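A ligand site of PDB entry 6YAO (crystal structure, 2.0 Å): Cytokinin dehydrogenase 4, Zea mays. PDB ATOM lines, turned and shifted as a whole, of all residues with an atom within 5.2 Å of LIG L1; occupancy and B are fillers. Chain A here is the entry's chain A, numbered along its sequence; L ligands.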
ATOM      1  N   PHE A  57      18.337 -18.217   2.755  1.00  0.00           N
ATOM      2  CA  PHE A  57      18.334 -18.006   4.209  1.00  0.00           C
ATOM      3  C   PHE A  57      16.947 -17.598   4.759  1.00  0.00           C
ATOM      4  O   PHE A  57      16.646 -17.895   5.926  1.00  0.00           O
ATOM      5  CB  PHE A  57      19.401 -16.984   4.559  1.00  0.00           C
ATOM      6  CG  PHE A  57      19.616 -16.731   6.027  1.00  0.00           C
ATOM      7  CD1 PHE A  57      20.403 -17.595   6.792  1.00  0.00           C
ATOM      8  CD2 PHE A  57      19.106 -15.575   6.633  1.00  0.00           C
ATOM      9  CE1 PHE A  57      20.684 -17.310   8.127  1.00  0.00           C
ATOM     10  CE2 PHE A  57      19.396 -15.291   7.964  1.00  0.00           C
ATOM     11  CZ  PHE A  57      20.186 -16.151   8.712  1.00  0.00           C
ATOM     12  N   ASP A 170      28.425  -7.125   8.587  1.00  0.00           N
ATOM     13  CA  ASP A 170      28.600  -7.724   9.920  1.00  0.00           C
ATOM     14  C   ASP A 170      28.982  -9.214   9.744  1.00  0.00           C
ATOM     15  O   ASP A 170      29.660  -9.784  10.586  1.00  0.00           O
ATOM     16  CB  ASP A 170      27.257  -7.704  10.727  1.00  0.00           C
ATOM     17  CG  ASP A 170      26.674  -6.362  11.115  1.00  0.00           C
ATOM     18  OD1 ASP A 170      27.418  -5.352  11.059  1.00  0.00           O
ATOM     19  OD2 ASP A 170      25.479  -6.319  11.456  1.00  0.00           O
ATOM     20  N   ILE A 185      26.639  -3.105   4.135  1.00  0.00           N
ATOM     21  CA  ILE A 185      26.659  -2.171   5.271  1.00  0.00           C
ATOM     22  C   ILE A 185      27.091  -2.820   6.600  1.00  0.00           C
ATOM     23  O   ILE A 185      26.655  -3.922   6.907  1.00  0.00           O
ATOM     24  CB  ILE A 185      25.239  -1.536   5.438  1.00  0.00           C
ATOM     25  CG1 ILE A 185      24.697  -0.948   4.085  1.00  0.00           C
ATOM     26  CG2 ILE A 185      25.223  -0.455   6.538  1.00  0.00           C
ATOM     27  CD1 ILE A 185      23.164  -0.607   4.133  1.00  0.00           C
ATOM     28  N   SER A 186      27.829  -2.049   7.414  1.00  0.00           N
ATOM     29  CA  SER A 186      28.253  -2.358   8.779  1.00  0.00           C
ATOM     30  C   SER A 186      28.632  -1.051   9.481  1.00  0.00           C
ATOM     31  O   SER A 186      28.373   0.017   8.943  1.00  0.00           O
ATOM     32  CB  SER A 186      29.402  -3.370   8.798  1.00  0.00           C
ATOM     33  OG  SER A 186      29.632  -3.839  10.118  1.00  0.00           O
ATOM     34  N   GLU A 285      27.880   1.034  15.805  1.00  0.00           N
ATOM     35  CA  GLU A 285      26.622   0.318  15.706  1.00  0.00           C
ATOM     36  C   GLU A 285      25.846   0.482  17.014  1.00  0.00           C
ATOM     37  O   GLU A 285      26.209   1.271  17.884  1.00  0.00           O
ATOM     38  CB  GLU A 285      26.768  -1.150  15.282  1.00  0.00           C
ATOM     39  CG  GLU A 285      27.135  -1.317  13.824  1.00  0.00           C
ATOM     40  CD  GLU A 285      26.913  -2.690  13.254  1.00  0.00           C
ATOM     41  OE1 GLU A 285      27.510  -2.983  12.200  1.00  0.00           O
ATOM     42  OE2 GLU A 285      26.167  -3.496  13.861  1.00  0.00           O
ATOM     43  N   VAL A 370      30.257 -12.792  13.815  1.00  0.00           N
ATOM     44  CA  VAL A 370      28.909 -13.307  13.508  1.00  0.00           C
ATOM     45  C   VAL A 370      28.985 -14.791  13.076  1.00  0.00           C
ATOM     46  O   VAL A 370      28.074 -15.574  13.376  1.00  0.00           O
ATOM     47  CB  VAL A 370      28.097 -12.401  12.515  1.00  0.00           C
ATOM     48  CG1 VAL A 370      26.691 -12.950  12.246  1.00  0.00           C
ATOM     49  CG2 VAL A 370      28.010 -10.968  13.054  1.00  0.00           C
ATOM     50  N   ALA A 373      28.632 -16.708  16.267  1.00  0.00           N
ATOM     51  CA  ALA A 373      27.224 -16.724  16.670  1.00  0.00           C
ATOM     52  C   ALA A 373      26.499 -17.802  15.833  1.00  0.00           C
ATOM     53  O   ALA A 373      25.681 -18.553  16.369  1.00  0.00           O
ATOM     54  CB  ALA A 373      26.600 -15.351  16.437  1.00  0.00           C
ATOM     55  N   GLU A 374      26.874 -17.915  14.530  1.00  0.00           N
ATOM     56  CA  GLU A 374      26.337 -18.921  13.606  1.00  0.00           C
ATOM     57  C   GLU A 374      26.638 -20.355  14.085  1.00  0.00           C
ATOM     58  O   GLU A 374      25.728 -21.185  14.089  1.00  0.00           O
ATOM     59  CB  GLU A 374      26.877 -18.697  12.170  1.00  0.00           C
ATOM     60  CG  GLU A 374      26.544 -19.820  11.196  1.00  0.00           C
ATOM     61  CD  GLU A 374      27.224 -19.789   9.846  1.00  0.00           C
ATOM     62  OE1 GLU A 374      28.033 -18.852   9.602  1.00  0.00           O
ATOM     63  OE2 GLU A 374      26.958 -20.695   9.027  1.00  0.00           O
ATOM     64  N   LEU A 377      24.468 -21.423  16.909  1.00  0.00           N
ATOM     65  CA  LEU A 377      23.091 -21.598  16.438  1.00  0.00           C
ATOM     66  C   LEU A 377      22.909 -22.942  15.749  1.00  0.00           C
ATOM     67  O   LEU A 377      21.878 -23.592  15.931  1.00  0.00           O
ATOM     68  CB  LEU A 377      22.644 -20.444  15.505  1.00  0.00           C
ATOM     69  CG  LEU A 377      22.339 -19.099  16.183  1.00  0.00           C
ATOM     70  CD1 LEU A 377      22.357 -17.957  15.173  1.00  0.00           C
ATOM     71  CD2 LEU A 377      21.003 -19.133  16.933  1.00  0.00           C
ATOM     72  N   TRP A 383      19.665 -22.529  13.189  1.00  0.00           N
ATOM     73  CA  TRP A 383      20.214 -21.778  12.068  1.00  0.00           C
ATOM     74  C   TRP A 383      19.375 -21.985  10.831  1.00  0.00           C
ATOM     75  O   TRP A 383      19.020 -21.011  10.181  1.00  0.00           O
ATOM     76  CB  TRP A 383      21.682 -22.159  11.816  1.00  0.00           C
ATOM     77  CG  TRP A 383      22.312 -21.455  10.651  1.00  0.00           C
ATOM     78  CD1 TRP A 383      22.529 -21.959   9.400  1.00  0.00           C
ATOM     79  CD2 TRP A 383      22.817 -20.103  10.619  1.00  0.00           C
ATOM     80  NE1 TRP A 383      23.170 -21.037   8.613  1.00  0.00           N
ATOM     81  CE2 TRP A 383      23.356 -19.875   9.339  1.00  0.00           C
ATOM     82  CE3 TRP A 383      22.834 -19.055  11.557  1.00  0.00           C
ATOM     83  CZ2 TRP A 383      23.904 -18.649   8.956  1.00  0.00           C
ATOM     84  CZ3 TRP A 383      23.418 -17.850  11.199  1.00  0.00           C
ATOM     85  CH2 TRP A 383      23.931 -17.648   9.910  1.00  0.00           C
ATOM     86  N   TRP A 389      13.465 -11.498   7.927  1.00  0.00           N
ATOM     87  CA  TRP A 389      14.238 -10.295   8.219  1.00  0.00           C
ATOM     88  C   TRP A 389      13.720  -9.060   7.511  1.00  0.00           C
ATOM     89  O   TRP A 389      13.422  -9.088   6.301  1.00  0.00           O
ATOM     90  CB  TRP A 389      15.722 -10.504   7.903  1.00  0.00           C
ATOM     91  CG  TRP A 389      16.417 -11.407   8.883  1.00  0.00           C
ATOM     92  CD1 TRP A 389      15.850 -12.098   9.930  1.00  0.00           C
ATOM     93  CD2 TRP A 389      17.832 -11.691   8.941  1.00  0.00           C
ATOM     94  NE1 TRP A 389      16.825 -12.752  10.642  1.00  0.00           N
ATOM     95  CE2 TRP A 389      18.050 -12.496  10.073  1.00  0.00           C
ATOM     96  CE3 TRP A 389      18.941 -11.261   8.197  1.00  0.00           C
ATOM     97  CZ2 TRP A 389      19.324 -12.913  10.463  1.00  0.00           C
ATOM     98  CZ3 TRP A 389      20.201 -11.699   8.557  1.00  0.00           C
ATOM     99  CH2 TRP A 389      20.383 -12.495   9.685  1.00  0.00           C
ATOM    100  N   ASN A 391      14.743  -4.902   6.952  1.00  0.00           N
ATOM    101  CA  ASN A 391      15.754  -3.857   7.101  1.00  0.00           C
ATOM    102  C   ASN A 391      15.249  -2.574   6.536  1.00  0.00           C
ATOM    103  O   ASN A 391      14.914  -2.517   5.350  1.00  0.00           O
ATOM    104  CB  ASN A 391      17.085  -4.279   6.391  1.00  0.00           C
ATOM    105  CG  ASN A 391      17.598  -5.578   6.924  1.00  0.00           C
ATOM    106  OD1 ASN A 391      18.177  -5.619   7.998  1.00  0.00           O
ATOM    107  ND2 ASN A 391      17.341  -6.680   6.241  1.00  0.00           N
ATOM    108  N   PRO A 421      18.187 -10.376  17.155  1.00  0.00           N
ATOM    109  CA  PRO A 421      18.526  -8.968  17.423  1.00  0.00           C
ATOM    110  C   PRO A 421      17.803  -7.914  16.557  1.00  0.00           C
ATOM    111  O   PRO A 421      17.272  -8.202  15.485  1.00  0.00           O
ATOM    112  CB  PRO A 421      20.044  -8.924  17.199  1.00  0.00           C
ATOM    113  CG  PRO A 421      20.320  -9.995  16.220  1.00  0.00           C
ATOM    114  CD  PRO A 421      19.258 -11.054  16.393  1.00  0.00           C
ATOM    115  N   LEU A 423      19.057  -4.282  15.335  1.00  0.00           N
ATOM    116  CA  LEU A 423      20.187  -3.346  15.244  1.00  0.00           C
ATOM    117  C   LEU A 423      19.741  -1.972  14.784  1.00  0.00           C
ATOM    118  O   LEU A 423      18.753  -1.853  14.041  1.00  0.00           O
ATOM    119  CB  LEU A 423      21.324  -3.898  14.309  1.00  0.00           C
ATOM    120  CG  LEU A 423      21.771  -5.380  14.492  1.00  0.00           C
ATOM    121  CD1 LEU A 423      23.001  -5.679  13.635  1.00  0.00           C
ATOM    122  CD2 LEU A 423      22.092  -5.711  15.920  1.00  0.00           C
ATOM    123  N   TYR A 425      21.622   2.101  13.940  1.00  0.00           N
ATOM    124  CA  TYR A 425      22.725   3.049  13.907  1.00  0.00           C
ATOM    125  C   TYR A 425      22.595   4.020  12.720  1.00  0.00           C
ATOM    126  O   TYR A 425      22.108   3.632  11.659  1.00  0.00           O
ATOM    127  CB  TYR A 425      24.113   2.336  13.916  1.00  0.00           C
ATOM    128  CG  TYR A 425      24.310   1.270  12.866  1.00  0.00           C
ATOM    129  CD1 TYR A 425      23.906  -0.040  13.083  1.00  0.00           C
ATOM    130  CD2 TYR A 425      24.950   1.562  11.662  1.00  0.00           C
ATOM    131  CE1 TYR A 425      24.106  -1.036  12.113  1.00  0.00           C
ATOM    132  CE2 TYR A 425      25.205   0.572  10.714  1.00  0.00           C
ATOM    133  CZ  TYR A 425      24.803  -0.735  10.956  1.00  0.00           C
ATOM    134  OH  TYR A 425      25.065  -1.688  10.004  1.00  0.00           O
ATOM    135  N   LEU A 448      19.910   2.831   9.771  1.00  0.00           N
ATOM    136  CA  LEU A 448      19.582   1.484   9.349  1.00  0.00           C
ATOM    137  C   LEU A 448      18.962   0.872  10.588  1.00  0.00           C
ATOM    138  O   LEU A 448      19.535   0.922  11.679  1.00  0.00           O
ATOM    139  CB  LEU A 448      20.804   0.673   8.901  1.00  0.00           C
ATOM    140  CG  LEU A 448      20.602  -0.882   8.715  1.00  0.00           C
ATOM    141  CD1 LEU A 448      19.466  -1.227   7.701  1.00  0.00           C
ATOM    142  CD2 LEU A 448      21.925  -1.543   8.283  1.00  0.00           C
ATOM    143  N   ALA A 450      17.619  -2.723  11.589  1.00  0.00           N
ATOM    144  CA  ALA A 450      17.607  -4.123  11.124  1.00  0.00           C
ATOM    145  C   ALA A 450      16.884  -5.045  12.106  1.00  0.00           C
ATOM    146  O   ALA A 450      17.361  -5.284  13.225  1.00  0.00           O
ATOM    147  CB  ALA A 450      19.057  -4.605  10.873  1.00  0.00           C
ATOM    148  N   LEU A 452      16.226  -8.474  12.814  1.00  0.00           N
ATOM    149  CA  LEU A 452      16.834  -9.767  12.458  1.00  0.00           C
ATOM    150  C   LEU A 452      16.295 -10.913  13.318  1.00  0.00           C
ATOM    151  O   LEU A 452      17.040 -11.563  14.041  1.00  0.00           O
ATOM    152  CB  LEU A 452      18.379  -9.659  12.543  1.00  0.00           C
ATOM    153  CG  LEU A 452      19.020  -8.459  11.847  1.00  0.00           C
ATOM    154  CD1 LEU A 452      20.480  -8.446  12.066  1.00  0.00           C
ATOM    155  CD2 LEU A 452      18.700  -8.442  10.328  1.00  0.00           C
ATOM    156  N   TYR A 487      15.913  -1.589   2.763  1.00  0.00           N
ATOM    157  CA  TYR A 487      17.212  -2.072   2.321  1.00  0.00           C
ATOM    158  C   TYR A 487      16.916  -3.569   2.018  1.00  0.00           C
ATOM    159  O   TYR A 487      16.162  -4.193   2.762  1.00  0.00           O
ATOM    160  CB  TYR A 487      18.295  -1.915   3.414  1.00  0.00           C
ATOM    161  CG  TYR A 487      19.631  -2.543   3.033  1.00  0.00           C
ATOM    162  CD1 TYR A 487      20.225  -2.271   1.800  1.00  0.00           C
ATOM    163  CD2 TYR A 487      20.309  -3.375   3.918  1.00  0.00           C
ATOM    164  CE1 TYR A 487      21.458  -2.848   1.442  1.00  0.00           C
ATOM    165  CE2 TYR A 487      21.553  -3.936   3.583  1.00  0.00           C
ATOM    166  CZ  TYR A 487      22.122  -3.675   2.343  1.00  0.00           C
ATOM    167  OH  TYR A 487      23.330  -4.225   2.005  1.00  0.00           O
ATOM    168  N   LEU A 488      17.449  -4.121   0.903  1.00  0.00           N
ATOM    169  CA  LEU A 488      17.162  -5.486   0.383  1.00  0.00           C
ATOM    170  C   LEU A 488      15.635  -5.524   0.095  1.00  0.00           C
ATOM    171  O   LEU A 488      14.921  -6.346   0.699  1.00  0.00           O
ATOM    172  CB  LEU A 488      17.584  -6.598   1.404  1.00  0.00           C
ATOM    173  CG  LEU A 488      18.988  -6.452   2.040  1.00  0.00           C
ATOM    174  CD1 LEU A 488      19.215  -7.460   3.103  1.00  0.00           C
ATOM    175  CD2 LEU A 488      20.050  -6.515   1.000  1.00  0.00           C
HETATM  176  F1  LIG L   1      23.280 -14.011  11.737  1.00  0.00           F
HETATM  177  C1  LIG L   1      22.896 -14.176  13.020  1.00  0.00           C
HETATM  178  F2  LIG L   1      23.898 -14.611  13.785  1.00  0.00           F
HETATM  179  F3  LIG L   1      21.873 -15.032  13.043  1.00  0.00           F
HETATM  180  O1  LIG L   1      22.432 -12.967  13.567  1.00  0.00           O
HETATM  181  C2  LIG L   1      23.315 -11.862  13.601  1.00  0.00           C
HETATM  182  C3  LIG L   1      23.324 -10.973  12.527  1.00  0.00           C
HETATM  183  C4  LIG L   1      23.995 -11.552  14.772  1.00  0.00           C
HETATM  184  C5  LIG L   1      24.700 -10.367  14.859  1.00  0.00           C
HETATM  185  C6  LIG L   1      24.738  -9.486  13.777  1.00  0.00           C
HETATM  186  C7  LIG L   1      24.128  -9.834  12.561  1.00  0.00           C
HETATM  187  N1  LIG L   1      24.078  -8.841  11.558  1.00  0.00           N
HETATM  188  C8  LIG L   1      23.305  -8.848  10.384  1.00  0.00           C
HETATM  189  O2  LIG L   1      22.698  -9.824   9.997  1.00  0.00           O
HETATM  190  N2  LIG L   1      23.277  -7.610   9.696  1.00  0.00           N
HETATM  191  C9  LIG L   1      22.535  -7.272   8.524  1.00  0.00           C
HETATM  192  C10 LIG L   1      21.604  -8.141   7.922  1.00  0.00           C
HETATM  193  C11 LIG L   1      20.876  -7.743   6.805  1.00  0.00           C
HETATM  194  C12 LIG L   1      20.999  -6.440   6.315  1.00  0.00           C
HETATM  195  C13 LIG L   1      21.862  -5.555   6.964  1.00  0.00           C
HETATM  196  C14 LIG L   1      22.595  -5.934   8.090  1.00  0.00           C
HETATM  197  C15 LIG L   1      23.519  -4.934   8.759  1.00  0.00           C
HETATM  198  C16 LIG L   1      23.030  -4.510  10.129  1.00  0.00           C
HETATM  199  O3  LIG L   1      24.135  -4.020  10.869  1.00  0.00           O
HETATM  200  P1  LG2 L   2      22.431 -13.852  -2.966  1.00  0.00           P
HETATM  201  O1  LG2 L   2      21.473 -13.808  -1.830  1.00  0.00           O
HETATM  202  O2  LG2 L   2      22.696 -15.252  -3.548  1.00  0.00           O
HETATM  203  O3  LG2 L   2      22.033 -12.861  -4.174  1.00  0.00           O
HETATM  204  C1  LG2 L   2      21.320 -11.625  -3.900  1.00  0.00           C
HETATM  205  C2  LG2 L   2      20.941 -10.974  -5.214  1.00  0.00           C
HETATM  206  O4  LG2 L   2      22.139 -10.640  -5.944  1.00  0.00           O
HETATM  207  C3  LG2 L   2      20.112 -11.845  -6.151  1.00  0.00           C
HETATM  208  O5  LG2 L   2      19.215 -11.053  -6.919  1.00  0.00           O
HETATM  209  C4  LG2 L   2      21.192 -12.526  -7.007  1.00  0.00           C
HETATM  210  O6  LG2 L   2      20.719 -13.049  -8.254  1.00  0.00           O
HETATM  211  C5  LG2 L   2      22.199 -11.383  -7.149  1.00  0.00           C
HETATM  212  N1  LG2 L   2      23.586 -11.782  -7.363  1.00  0.00           N
HETATM  213  C6  LG2 L   2      24.339 -12.684  -6.647  1.00  0.00           C
HETATM  214  N2  LG2 L   2      25.595 -12.728  -7.002  1.00  0.00           N
HETATM  215  C7  LG2 L   2      25.684 -11.821  -8.047  1.00  0.00           C
HETATM  216  C8  LG2 L   2      26.749 -11.421  -8.881  1.00  0.00           C
HETATM  217  N3  LG2 L   2      27.987 -11.926  -8.819  1.00  0.00           N
HETATM  218  N4  LG2 L   2      26.490 -10.466  -9.812  1.00  0.00           N
HETATM  219  C9  LG2 L   2      25.259  -9.952  -9.883  1.00  0.00           C
HETATM  220  N5  LG2 L   2      24.186 -10.255  -9.168  1.00  0.00           N
HETATM  221  C10 LG2 L   2      24.452 -11.211  -8.267  1.00  0.00           C
HETATM  222  N6  LG2 L   2      23.959  -7.305   4.390  1.00  0.00           N
HETATM  223  C11 LG2 L   2      24.648  -6.196   4.774  1.00  0.00           C
HETATM  224  O7  LG2 L   2      24.724  -5.196   4.050  1.00  0.00           O
HETATM  225  N7  LG2 L   2      25.278  -6.170   6.001  1.00  0.00           N
HETATM  226  C12 LG2 L   2      25.329  -7.216   6.910  1.00  0.00           C
HETATM  227  O8  LG2 L   2      25.900  -7.056   7.963  1.00  0.00           O
HETATM  228  C13 LG2 L   2      24.635  -8.396   6.486  1.00  0.00           C
HETATM  229  N8  LG2 L   2      24.652  -9.446   7.281  1.00  0.00           N
HETATM  230  C14 LG2 L   2      24.010 -10.599   6.854  1.00  0.00           C
HETATM  231  C15 LG2 L   2      24.059 -11.740   7.660  1.00  0.00           C
HETATM  232  C16 LG2 L   2      23.415 -12.920   7.292  1.00  0.00           C
HETATM  233  C17 LG2 L   2      23.412 -14.094   8.239  1.00  0.00           C
HETATM  234  C18 LG2 L   2      22.717 -12.970   6.062  1.00  0.00           C
HETATM  235  C19 LG2 L   2      22.039 -14.230   5.596  1.00  0.00           C
HETATM  236  C20 LG2 L   2      22.680 -11.838   5.256  1.00  0.00           C
HETATM  237  C21 LG2 L   2      23.298 -10.645   5.640  1.00  0.00           C
HETATM  238  N9  LG2 L   2      23.252  -9.463   4.843  1.00  0.00           N
HETATM  239  C22 LG2 L   2      23.943  -8.351   5.210  1.00  0.00           C
HETATM  240  C23 LG2 L   2      22.447  -9.419   3.608  1.00  0.00           C
HETATM  241  C24 LG2 L   2      23.223  -9.720   2.332  1.00  0.00           C
HETATM  242  O9  LG2 L   2      24.009  -8.584   1.969  1.00  0.00           O
HETATM  243  C25 LG2 L   2      22.279 -10.077   1.186  1.00  0.00           C
HETATM  244  O10 LG2 L   2      21.643 -11.322   1.504  1.00  0.00           O
HETATM  245  C26 LG2 L   2      22.827 -10.153  -0.237  1.00  0.00           C
HETATM  246  O11 LG2 L   2      21.827 -10.720  -1.088  1.00  0.00           O
HETATM  247  C27 LG2 L   2      24.160 -10.867  -0.385  1.00  0.00           C
HETATM  248  O12 LG2 L   2      24.061 -12.265  -0.036  1.00  0.00           O
HETATM  249  P2  LG2 L   2      24.632 -13.372  -1.099  1.00  0.00           P
HETATM  250  O13 LG2 L   2      26.074 -13.253  -1.381  1.00  0.00           O
HETATM  251  O14 LG2 L   2      24.290 -14.742  -0.539  1.00  0.00           O
HETATM  252  O15 LG2 L   2      23.831 -13.240  -2.477  1.00  0.00           O
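Ile 185 touches LIG L1 (O to C15, 3.8 Å).
Glu 285 touches LIG L1 (OE2 to O3, 3.7 Å).
CG1 of Val 370 touches F2 of LIG L1 (3.6 Å).
Ala 373 touches LIG L1 (CB to F2, 3.9 Å).
Leu 377 touches LIG L1.
Trp 383 touches LIG L1.
Trp 389 touches LIG L1.
OD1 of Asn 391 touches C12 of LIG L1, 3.4 Å away.
Leu 423 touches LIG L1.
CD2 of Leu 448 touches C16 of LIG L1, 3.7 Å away.
Leu 452 touches LIG L1.
Tyr 487 touches LIG L1 (CE2 to C12, 3.7 Å).
CD1 of Leu 488 touches C12 of LIG L1, at 3.8 Å.
Hydrophobic or aromatic side chains within 4 Å of LIG L1: Val 370, Ala 373, Leu 377, Trp 383, Trp 389, Leu 423, Tyr 425, Leu 448, Leu 452, Tyr 487 and Leu 488.
15 residues have an atom within 4 Å of LIG L1: Asp 170, Ile 185, Glu 285, Val 370, Ala 373, Leu 377, Trp 383, Trp 389, Asn 391, Leu 423, Tyr 425, Leu 448, Leu 452, Tyr 487 and Leu 488.
The nearest printed residue that does not touch LIG L1 is Ala 450 (4.04 Å).
O of Tyr 425 lies within hydrogen-bond range of N of Leu 448.
The side-chain carboxylate (OE1) of Glu 285 lies close to the side-chain carboxylate (OD1) of Asp 170, 2.6 Å away.
The side-chain hydroxyl of Ser 186 sits at hydrogen-bond distance from the side-chain carboxylate of Asp 170 (2.8 Å).
The backbone NH of Leu 452 sits at hydrogen-bond distance from the backbone carbonyl oxygen of Pro 421, at 2.9 Å.
The backbone NH (N) of Tyr 487 sits at hydrogen-bond distance from the backbone carbonyl oxygen (O) of Asn 391 (2.9 Å).
The backbone carbonyl oxygen (O) of Leu 423 sits at hydrogen-bond distance from the backbone NH (N) of Ala 450 (2.8 Å).
OE1 of Glu 285 sits at hydrogen-bond distance from OG of Ser 186.
The side-chain hydroxyl (OH) of Tyr 425 sits at hydrogen-bond distance from an oxygen (O3) of LIG L1.
An oxygen (O3) of LIG L1 sits at hydrogen-bond distance from the side-chain carboxylate of Asp 170.
An oxygen (O8) of LG2 L2 is in hydrogen-bond range of the backbone NH (N) of Asp 170, at 2.6 Å.
OH of Tyr 487 lies within hydrogen-bond range of O7 of LG2 L2 (2.7 Å).
N of Ile 185 sits at hydrogen-bond distance from O7 of LG2 L2, at 2.8 Å.
The backbone carbonyl oxygen (O) of Ile 185 lies within hydrogen-bond range of a nitrogen (N7) of LG2 L2 (2.8 Å).
O8 of LG2 L2 is in hydrogen-bond range of N2 of LIG L1.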
